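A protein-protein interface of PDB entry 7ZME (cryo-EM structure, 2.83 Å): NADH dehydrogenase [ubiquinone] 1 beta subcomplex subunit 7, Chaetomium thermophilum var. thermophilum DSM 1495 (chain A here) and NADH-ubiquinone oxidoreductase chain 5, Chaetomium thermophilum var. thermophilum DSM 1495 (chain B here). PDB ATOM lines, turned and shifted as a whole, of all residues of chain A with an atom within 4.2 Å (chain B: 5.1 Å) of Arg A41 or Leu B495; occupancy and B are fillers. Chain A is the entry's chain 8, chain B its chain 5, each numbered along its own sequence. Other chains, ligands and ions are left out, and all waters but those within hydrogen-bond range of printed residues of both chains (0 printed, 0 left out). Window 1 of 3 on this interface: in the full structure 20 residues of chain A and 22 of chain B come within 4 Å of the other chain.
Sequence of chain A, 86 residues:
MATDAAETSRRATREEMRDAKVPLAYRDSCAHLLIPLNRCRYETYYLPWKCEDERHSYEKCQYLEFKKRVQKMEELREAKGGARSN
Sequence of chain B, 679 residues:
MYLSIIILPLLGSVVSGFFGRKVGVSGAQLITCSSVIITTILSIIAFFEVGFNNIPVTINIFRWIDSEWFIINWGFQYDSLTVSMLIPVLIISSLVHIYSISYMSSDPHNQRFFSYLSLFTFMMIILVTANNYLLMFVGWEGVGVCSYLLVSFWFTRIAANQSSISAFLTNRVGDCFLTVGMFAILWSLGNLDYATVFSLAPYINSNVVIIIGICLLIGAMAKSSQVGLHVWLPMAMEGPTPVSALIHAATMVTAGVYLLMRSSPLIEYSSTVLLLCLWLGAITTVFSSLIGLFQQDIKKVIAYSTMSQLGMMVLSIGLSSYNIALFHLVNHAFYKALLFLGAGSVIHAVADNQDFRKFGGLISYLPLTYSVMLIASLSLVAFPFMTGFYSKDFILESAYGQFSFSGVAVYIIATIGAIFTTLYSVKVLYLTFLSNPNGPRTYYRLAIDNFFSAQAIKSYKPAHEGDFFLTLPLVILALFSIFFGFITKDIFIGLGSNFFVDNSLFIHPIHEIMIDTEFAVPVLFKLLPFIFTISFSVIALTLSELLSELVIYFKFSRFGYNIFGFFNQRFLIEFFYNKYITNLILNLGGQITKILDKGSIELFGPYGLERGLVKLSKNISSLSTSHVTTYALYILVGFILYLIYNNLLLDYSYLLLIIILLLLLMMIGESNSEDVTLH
Among the printed residues, pairs that only touch across the chains: Tyr A46 with Asp B490 (3.2 Å), Tyr A26 with Met B514 (3.2 Å), Gln A62 with Leu B495 (3.3 Å), Gln A62 with Phe B519 (3.4 Å), Tyr A58 with Leu B495 (3.5 Å), Tyr A26 with Gly B496 (3.5 Å), Glu A59 with Leu B495 (3.7 Å), Glu A59 with Phe B519 (3.8 Å), Arg A41 with Gly B494 (3.99 Å) and Asn A38 with Ser B497 (3.99 Å).
Printed residues of chain B within 4 Å of Tyr A26: Leu B495 (3.0 Å), Gly B496 (3.5 Å) and Met B514 (3.2 Å). Of the printed residues of chain B, Arg A41 touches Asp B490, Gly B494, Leu B495, Gly B496 and Ser B497. Thr A44 touches none of the printed residues of chain B. Of the printed residues of chain B, Gln A62 touches Leu B495 (3.3 Å) and Phe B519 (3.4 Å). Leu B495 touches just these residues of chain A: Tyr A26 (3.0 Å), Arg A41 (3.4 Å), Tyr A58 (3.5 Å), Glu A59 (3.7 Å) and Gln A62 (3.3 Å). Printed residues of chain A within 4 Å of Asn B498: Asn A38 and Tyr A46. The nearest printed residue of chain B that does not touch Tyr A26 is Ser B497 (4.9 Å).
Of the 14 printed residues of chain A, 7 touch a printed residue of chain B. Hydrophobic or aromatic side chains of chain A within 4 Å of the printed part of chain B: Tyr A26, Tyr A46 and Tyr A58. Among the printed residues, 19 pairs touch across the chains. Among the printed residues, Asp or Glu carboxylates within 4 Å of a Lys or Arg side-chain nitrogen of the other chain: Arg A41 with Asp B490.
The side-chain carboxylate (OD1) of Asp B490 lies within salt-bridge range of the guanidinium group (NE) of Arg A41 (3.2 Å). The backbone carbonyl oxygen of Leu B495 sits at hydrogen-bond distance from the side-chain hydroxyl of Tyr A26, at 3.0 Å. O of Gly B496 lies close to OD1 of Asn A38 (2.9 Å). NH2 of Arg A41 lies close to O of Gly B496 (3.3 Å). The side-chain amide nitrogen (ND2) of Asn B498 sits close to the side-chain amide nitrogen (ND2) of Asn A38, 3.3 Å away. The side-chain amide oxygen (OD1) of Asn B498 sits at hydrogen-bond distance from the side-chain hydroxyl (OH) of Tyr A46. The backbone NH of Leu B495 sits close to the guanidinium group of Arg A41, at 3.4 Å. NH2 of Arg A41 sits close to N of Ser B497 (3.3 Å). The side-chain carboxylate (OE2) of Glu B518 sits close to the side-chain carboxylate (OE1) of Glu A59.
The guanidinium group (NH2) of Arg A41 is in hydrogen-bond range of the side-chain amide oxygen (OD1) of Asn A38, at 2.7 Å. O of Arg A41 sits at hydrogen-bond distance from N of Tyr A46, at 2.8 Å. OH of Tyr A58 lies close to OE1 of Gln A62, 3.3 Å away.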
ATOM      1  N   TYR A  26      -4.330  -5.719  -7.894  1.00  0.00           N
ATOM      2  CA  TYR A  26      -5.304  -6.746  -8.230  1.00  0.00           C
ATOM      3  C   TYR A  26      -6.422  -6.198  -9.110  1.00  0.00           C
ATOM      4  O   TYR A  26      -7.480  -6.821  -9.231  1.00  0.00           O
ATOM      5  CB  TYR A  26      -5.860  -7.356  -6.947  1.00  0.00           C
ATOM      6  CG  TYR A  26      -4.808  -8.115  -6.178  1.00  0.00           C
ATOM      7  CD1 TYR A  26      -3.711  -8.663  -6.829  1.00  0.00           C
ATOM      8  CD2 TYR A  26      -4.875  -8.230  -4.799  1.00  0.00           C
ATOM      9  CE1 TYR A  26      -2.734  -9.339  -6.134  1.00  0.00           C
ATOM     10  CE2 TYR A  26      -3.898  -8.900  -4.094  1.00  0.00           C
ATOM     11  CZ  TYR A  26      -2.832  -9.455  -4.767  1.00  0.00           C
ATOM     12  OH  TYR A  26      -1.858 -10.126  -4.067  1.00  0.00           O
ATOM     13  N   LEU A  37     -15.142 -12.293  -2.782  1.00  0.00           N
ATOM     14  CA  LEU A  37     -14.202 -12.870  -1.826  1.00  0.00           C
ATOM     15  C   LEU A  37     -13.889 -11.902  -0.700  1.00  0.00           C
ATOM     16  O   LEU A  37     -13.809 -12.299   0.469  1.00  0.00           O
ATOM     17  CB  LEU A  37     -12.918 -13.295  -2.532  1.00  0.00           C
ATOM     18  CG  LEU A  37     -11.912 -13.954  -1.591  1.00  0.00           C
ATOM     19  CD1 LEU A  37     -12.479 -15.213  -1.008  1.00  0.00           C
ATOM     20  CD2 LEU A  37     -10.631 -14.261  -2.334  1.00  0.00           C
ATOM     21  N   ASN A  38     -13.706 -10.627  -1.030  1.00  0.00           N
ATOM     22  CA  ASN A  38     -13.414  -9.641  -0.005  1.00  0.00           C
ATOM     23  C   ASN A  38     -14.620  -9.321   0.859  1.00  0.00           C
ATOM     24  O   ASN A  38     -14.466  -8.635   1.874  1.00  0.00           O
ATOM     25  CB  ASN A  38     -12.873  -8.376  -0.657  1.00  0.00           C
ATOM     26  CG  ASN A  38     -11.432  -8.518  -1.091  1.00  0.00           C
ATOM     27  OD1 ASN A  38     -10.828  -9.576  -0.931  1.00  0.00           O
ATOM     28  ND2 ASN A  38     -10.874  -7.454  -1.643  1.00  0.00           N
ATOM     29  N   ARG A  39     -15.813  -9.791   0.485  1.00  0.00           N
ATOM     30  CA  ARG A  39     -16.985  -9.570   1.325  1.00  0.00           C
ATOM     31  C   ARG A  39     -17.115 -10.639   2.402  1.00  0.00           C
ATOM     32  O   ARG A  39     -17.495 -10.334   3.536  1.00  0.00           O
ATOM     33  CB  ARG A  39     -18.250  -9.506   0.470  1.00  0.00           C
ATOM     34  CG  ARG A  39     -18.281  -8.319  -0.473  1.00  0.00           C
ATOM     35  CD  ARG A  39     -19.544  -8.304  -1.312  1.00  0.00           C
ATOM     36  NE  ARG A  39     -20.729  -8.073  -0.491  1.00  0.00           N
ATOM     37  CZ  ARG A  39     -21.650  -8.996  -0.234  1.00  0.00           C
ATOM     38  NH1 ARG A  39     -21.522 -10.216  -0.735  1.00  0.00           N
ATOM     39  NH2 ARG A  39     -22.696  -8.699   0.522  1.00  0.00           N
ATOM     40  N   CYS A  40     -16.809 -11.898   2.074  1.00  0.00           N
ATOM     41  CA  CYS A  40     -16.709 -12.913   3.121  1.00  0.00           C
ATOM     42  C   CYS A  40     -15.674 -12.531   4.162  1.00  0.00           C
ATOM     43  O   CYS A  40     -15.904 -12.699   5.365  1.00  0.00           O
ATOM     44  CB  CYS A  40     -16.364 -14.280   2.537  1.00  0.00           C
ATOM     45  SG  CYS A  40     -17.669 -15.143   1.683  1.00  0.00           S
ATOM     46  N   ARG A  41     -14.524 -12.027   3.721  1.00  0.00           N
ATOM     47  CA  ARG A  41     -13.499 -11.623   4.668  1.00  0.00           C
ATOM     48  C   ARG A  41     -14.029 -10.542   5.595  1.00  0.00           C
ATOM     49  O   ARG A  41     -13.849 -10.609   6.816  1.00  0.00           O
ATOM     50  CB  ARG A  41     -12.260 -11.148   3.917  1.00  0.00           C
ATOM     51  CG  ARG A  41     -11.502 -12.277   3.245  1.00  0.00           C
ATOM     52  CD  ARG A  41     -10.754 -11.789   2.029  1.00  0.00           C
ATOM     53  NE  ARG A  41      -9.684 -12.707   1.660  1.00  0.00           N
ATOM     54  CZ  ARG A  41      -9.074 -12.701   0.482  1.00  0.00           C
ATOM     55  NH1 ARG A  41      -8.109 -13.573   0.228  1.00  0.00           N
ATOM     56  NH2 ARG A  41      -9.423 -11.817  -0.440  1.00  0.00           N
ATOM     57  N   TYR A  42     -14.730  -9.557   5.038  1.00  0.00           N
ATOM     58  CA  TYR A  42     -15.406  -8.570   5.872  1.00  0.00           C
ATOM     59  C   TYR A  42     -16.460  -9.228   6.754  1.00  0.00           C
ATOM     60  O   TYR A  42     -16.470  -9.043   7.975  1.00  0.00           O
ATOM     61  CB  TYR A  42     -16.034  -7.491   4.992  1.00  0.00           C
ATOM     62  CG  TYR A  42     -16.927  -6.530   5.739  1.00  0.00           C
ATOM     63  CD1 TYR A  42     -16.390  -5.522   6.527  1.00  0.00           C
ATOM     64  CD2 TYR A  42     -18.309  -6.626   5.650  1.00  0.00           C
ATOM     65  CE1 TYR A  42     -17.204  -4.638   7.207  1.00  0.00           C
ATOM     66  CE2 TYR A  42     -19.130  -5.748   6.326  1.00  0.00           C
ATOM     67  CZ  TYR A  42     -18.573  -4.755   7.103  1.00  0.00           C
ATOM     68  OH  TYR A  42     -19.387  -3.878   7.781  1.00  0.00           O
ATOM     69  N   GLU A  43     -17.346 -10.022   6.151  1.00  0.00           N
ATOM     70  CA  GLU A  43     -18.487 -10.554   6.885  1.00  0.00           C
ATOM     71  C   GLU A  43     -18.092 -11.634   7.885  1.00  0.00           C
ATOM     72  O   GLU A  43     -18.707 -11.732   8.952  1.00  0.00           O
ATOM     73  CB  GLU A  43     -19.526 -11.105   5.904  1.00  0.00           C
ATOM     74  CG  GLU A  43     -20.786 -11.650   6.562  1.00  0.00           C
ATOM     75  CD  GLU A  43     -21.588 -10.576   7.270  1.00  0.00           C
ATOM     76  OE1 GLU A  43     -21.484  -9.393   6.880  1.00  0.00           O
ATOM     77  OE2 GLU A  43     -22.324 -10.915   8.220  1.00  0.00           O
ATOM     78  N   THR A  44     -17.077 -12.437   7.578  1.00  0.00           N
ATOM     79  CA  THR A  44     -16.679 -13.545   8.435  1.00  0.00           C
ATOM     80  C   THR A  44     -15.411 -13.259   9.229  1.00  0.00           C
ATOM     81  O   THR A  44     -14.818 -14.191   9.778  1.00  0.00           O
ATOM     82  CB  THR A  44     -16.494 -14.818   7.608  1.00  0.00           C
ATOM     83  OG1 THR A  44     -15.542 -14.577   6.564  1.00  0.00           O
ATOM     84  CG2 THR A  44     -17.816 -15.250   6.992  1.00  0.00           C
ATOM     85  N   TYR A  45     -14.985 -11.996   9.298  1.00  0.00           N
ATOM     86  CA  TYR A  45     -13.785 -11.595  10.035  1.00  0.00           C
ATOM     87  C   TYR A  45     -12.549 -12.350   9.556  1.00  0.00           C
ATOM     88  O   TYR A  45     -11.712 -12.769  10.355  1.00  0.00           O
ATOM     89  CB  TYR A  45     -13.967 -11.773  11.541  1.00  0.00           C
ATOM     90  CG  TYR A  45     -14.993 -10.853  12.151  1.00  0.00           C
ATOM     91  CD1 TYR A  45     -14.916  -9.478  11.973  1.00  0.00           C
ATOM     92  CD2 TYR A  45     -16.041 -11.359  12.905  1.00  0.00           C
ATOM     93  CE1 TYR A  45     -15.854  -8.636  12.531  1.00  0.00           C
ATOM     94  CE2 TYR A  45     -16.982 -10.525  13.466  1.00  0.00           C
ATOM     95  CZ  TYR A  45     -16.886  -9.165  13.276  1.00  0.00           C
ATOM     96  OH  TYR A  45     -17.828  -8.337  13.838  1.00  0.00           O
ATOM     97  N   TYR A  46     -12.447 -12.538   8.241  1.00  0.00           N
ATOM     98  CA  TYR A  46     -11.248 -13.056   7.588  1.00  0.00           C
ATOM     99  C   TYR A  46     -10.859 -14.445   8.083  1.00  0.00           C
ATOM    100  O   TYR A  46      -9.723 -14.879   7.878  1.00  0.00           O
ATOM    101  CB  TYR A  46     -10.065 -12.097   7.766  1.00  0.00           C
ATOM    102  CG  TYR A  46     -10.166 -10.809   6.986  1.00  0.00           C
ATOM    103  CD1 TYR A  46     -11.058  -9.822   7.359  1.00  0.00           C
ATOM    104  CD2 TYR A  46      -9.353 -10.575   5.890  1.00  0.00           C
ATOM    105  CE1 TYR A  46     -11.154  -8.644   6.653  1.00  0.00           C
ATOM    106  CE2 TYR A  46      -9.437  -9.399   5.181  1.00  0.00           C
ATOM    107  CZ  TYR A  46     -10.340  -8.437   5.566  1.00  0.00           C
ATOM    108  OH  TYR A  46     -10.430  -7.261   4.861  1.00  0.00           O
ATOM    109  N   TYR A  58     -12.010 -18.085  -6.682  1.00  0.00           N
ATOM    110  CA  TYR A  58     -11.141 -16.972  -7.045  1.00  0.00           C
ATOM    111  C   TYR A  58      -9.707 -17.439  -7.233  1.00  0.00           C
ATOM    112  O   TYR A  58      -9.021 -16.993  -8.157  1.00  0.00           O
ATOM    113  CB  TYR A  58     -11.209 -15.872  -5.987  1.00  0.00           C
ATOM    114  CG  TYR A  58     -10.254 -14.730  -6.249  1.00  0.00           C
ATOM    115  CD1 TYR A  58     -10.485 -13.828  -7.276  1.00  0.00           C
ATOM    116  CD2 TYR A  58      -9.118 -14.561  -5.476  1.00  0.00           C
ATOM    117  CE1 TYR A  58      -9.614 -12.787  -7.519  1.00  0.00           C
ATOM    118  CE2 TYR A  58      -8.244 -13.523  -5.710  1.00  0.00           C
ATOM    119  CZ  TYR A  58      -8.494 -12.640  -6.734  1.00  0.00           C
ATOM    120  OH  TYR A  58      -7.621 -11.605  -6.969  1.00  0.00           O
ATOM    121  N   GLU A  59      -9.240 -18.339  -6.366  1.00  0.00           N
ATOM    122  CA  GLU A  59      -7.903 -18.893  -6.538  1.00  0.00           C
ATOM    123  C   GLU A  59      -7.806 -19.736  -7.801  1.00  0.00           C
ATOM    124  O   GLU A  59      -6.728 -19.836  -8.395  1.00  0.00           O
ATOM    125  CB  GLU A  59      -7.516 -19.725  -5.314  1.00  0.00           C
ATOM    126  CG  GLU A  59      -6.907 -18.918  -4.182  1.00  0.00           C
ATOM    127  CD  GLU A  59      -5.888 -19.711  -3.387  1.00  0.00           C
ATOM    128  OE1 GLU A  59      -5.176 -20.539  -3.992  1.00  0.00           O
ATOM    129  OE2 GLU A  59      -5.797 -19.504  -2.159  1.00  0.00           O
ATOM    130  N   GLN A  62      -7.288 -17.409 -10.668  1.00  0.00           N
ATOM    131  CA  GLN A  62      -5.894 -16.987 -10.606  1.00  0.00           C
ATOM    132  C   GLN A  62      -5.001 -17.944 -11.378  1.00  0.00           C
ATOM    133  O   GLN A  62      -4.062 -17.514 -12.056  1.00  0.00           O
ATOM    134  CB  GLN A  62      -5.425 -16.922  -9.151  1.00  0.00           C
ATOM    135  CG  GLN A  62      -6.111 -15.895  -8.272  1.00  0.00           C
ATOM    136  CD  GLN A  62      -5.872 -14.474  -8.721  1.00  0.00           C
ATOM    137  OE1 GLN A  62      -6.776 -13.820  -9.229  1.00  0.00           O
ATOM    138  NE2 GLN A  62      -4.654 -13.986  -8.533  1.00  0.00           N
ATOM    139  N   ASP B 490      -5.094 -14.958   6.717  1.00  0.00           N
ATOM    140  CA  ASP B 490      -5.878 -14.326   5.663  1.00  0.00           C
ATOM    141  C   ASP B 490      -5.815 -12.806   5.734  1.00  0.00           C
ATOM    142  O   ASP B 490      -5.849 -12.142   4.694  1.00  0.00           O
ATOM    143  CB  ASP B 490      -7.330 -14.791   5.735  1.00  0.00           C
ATOM    144  CG  ASP B 490      -7.956 -14.957   4.369  1.00  0.00           C
ATOM    145  OD1 ASP B 490      -7.514 -14.275   3.422  1.00  0.00           O
ATOM    146  OD2 ASP B 490      -8.891 -15.774   4.242  1.00  0.00           O
ATOM    147  N   ILE B 493      -1.677 -12.096   4.629  1.00  0.00           N
ATOM    148  CA  ILE B 493      -1.207 -12.685   3.384  1.00  0.00           C
ATOM    149  C   ILE B 493      -2.359 -12.764   2.396  1.00  0.00           C
ATOM    150  O   ILE B 493      -2.373 -12.042   1.392  1.00  0.00           O
ATOM    151  CB  ILE B 493      -0.585 -14.073   3.619  1.00  0.00           C
ATOM    152  CG1 ILE B 493       0.658 -13.949   4.498  1.00  0.00           C
ATOM    153  CG2 ILE B 493      -0.236 -14.730   2.294  1.00  0.00           C
ATOM    154  CD1 ILE B 493       1.553 -12.793   4.123  1.00  0.00           C
ATOM    155  N   GLY B 494      -3.338 -13.616   2.685  1.00  0.00           N
ATOM    156  CA  GLY B 494      -4.450 -13.842   1.788  1.00  0.00           C
ATOM    157  C   GLY B 494      -3.971 -14.095   0.375  1.00  0.00           C
ATOM    158  O   GLY B 494      -2.868 -14.603   0.140  1.00  0.00           O
ATOM    159  N   LEU B 495      -4.816 -13.748  -0.589  1.00  0.00           N
ATOM    160  CA  LEU B 495      -4.351 -13.671  -1.965  1.00  0.00           C
ATOM    161  C   LEU B 495      -4.859 -12.376  -2.581  1.00  0.00           C
ATOM    162  O   LEU B 495      -4.240 -11.832  -3.500  1.00  0.00           O
ATOM    163  CB  LEU B 495      -4.803 -14.897  -2.764  1.00  0.00           C
ATOM    164  CG  LEU B 495      -4.151 -15.118  -4.133  1.00  0.00           C
ATOM    165  CD1 LEU B 495      -4.092 -16.602  -4.447  1.00  0.00           C
ATOM    166  CD2 LEU B 495      -4.889 -14.386  -5.236  1.00  0.00           C
ATOM    167  N   GLY B 496      -5.984 -11.879  -2.076  1.00  0.00           N
ATOM    168  CA  GLY B 496      -6.539 -10.620  -2.527  1.00  0.00           C
ATOM    169  C   GLY B 496      -7.169  -9.820  -1.406  1.00  0.00           C
ATOM    170  O   GLY B 496      -8.082  -9.024  -1.645  1.00  0.00           O
ATOM    171  N   SER B 497      -6.692 -10.027  -0.181  1.00  0.00           N
ATOM    172  CA  SER B 497      -7.329  -9.427   0.983  1.00  0.00           C
ATOM    173  C   SER B 497      -7.256  -7.907   0.921  1.00  0.00           C
ATOM    174  O   SER B 497      -6.328  -7.328   0.352  1.00  0.00           O
ATOM    175  CB  SER B 497      -6.671  -9.937   2.265  1.00  0.00           C
ATOM    176  OG  SER B 497      -5.415  -9.323   2.479  1.00  0.00           O
ATOM    177  N   ASN B 498      -8.255  -7.259   1.513  1.00  0.00           N
ATOM    178  CA  ASN B 498      -8.407  -5.813   1.450  1.00  0.00           C
ATOM    179  C   ASN B 498      -8.277  -5.185   2.831  1.00  0.00           C
ATOM    180  O   ASN B 498      -8.980  -4.231   3.166  1.00  0.00           O
ATOM    181  CB  ASN B 498      -9.748  -5.423   0.835  1.00  0.00           C
ATOM    182  CG  ASN B 498     -10.911  -6.162   1.456  1.00  0.00           C
ATOM    183  OD1 ASN B 498     -10.737  -6.960   2.376  1.00  0.00           O
ATOM    184  ND2 ASN B 498     -12.116  -5.856   0.994  1.00  0.00           N
ATOM    185  N   MET B 514       2.943 -11.649  -5.671  1.00  0.00           N
ATOM    186  CA  MET B 514       2.103 -12.559  -4.899  1.00  0.00           C
ATOM    187  C   MET B 514       1.600 -13.718  -5.751  1.00  0.00           C
ATOM    188  O   MET B 514       1.614 -14.874  -5.314  1.00  0.00           O
ATOM    189  CB  MET B 514       0.929 -11.793  -4.288  1.00  0.00           C
ATOM    190  CG  MET B 514       0.058 -12.622  -3.367  1.00  0.00           C
ATOM    191  SD  MET B 514       0.963 -13.191  -1.921  1.00  0.00           S
ATOM    192  CE  MET B 514       1.120 -11.660  -1.006  1.00  0.00           C
ATOM    193  N   GLU B 518       2.700 -18.067  -5.381  1.00  0.00           N
ATOM    194  CA  GLU B 518       1.800 -19.188  -5.156  1.00  0.00           C
ATOM    195  C   GLU B 518       1.700 -20.123  -6.352  1.00  0.00           C
ATOM    196  O   GLU B 518       1.135 -21.214  -6.214  1.00  0.00           O
ATOM    197  CB  GLU B 518       0.406 -18.670  -4.794  1.00  0.00           C
ATOM    198  CG  GLU B 518      -0.404 -19.609  -3.915  1.00  0.00           C
ATOM    199  CD  GLU B 518      -1.440 -18.880  -3.082  1.00  0.00           C
ATOM    200  OE1 GLU B 518      -1.260 -17.670  -2.833  1.00  0.00           O
ATOM    201  OE2 GLU B 518      -2.436 -19.515  -2.678  1.00  0.00           O
ATOM    202  N   PHE B 519       2.231 -19.742  -7.504  1.00  0.00           N
ATOM    203  CA  PHE B 519       2.013 -20.542  -8.703  1.00  0.00           C
ATOM    204  C   PHE B 519       3.288 -20.922  -9.438  1.00  0.00           C
ATOM    205  O   PHE B 519       3.386 -22.044  -9.939  1.00  0.00           O
ATOM    206  CB  PHE B 519       1.090 -19.781  -9.653  1.00  0.00           C
ATOM    207  CG  PHE B 519      -0.319 -19.662  -9.164  1.00  0.00           C
ATOM    208  CD1 PHE B 519      -0.924 -20.704  -8.487  1.00  0.00           C
ATOM    209  CD2 PHE B 519      -1.041 -18.505  -9.384  1.00  0.00           C
ATOM    210  CE1 PHE B 519      -2.218 -20.593  -8.041  1.00  0.00           C
ATOM    211  CE2 PHE B 519      -2.332 -18.390  -8.939  1.00  0.00           C
ATOM    212  CZ  PHE B 519      -2.925 -19.434  -8.268  1.00  0.00           C
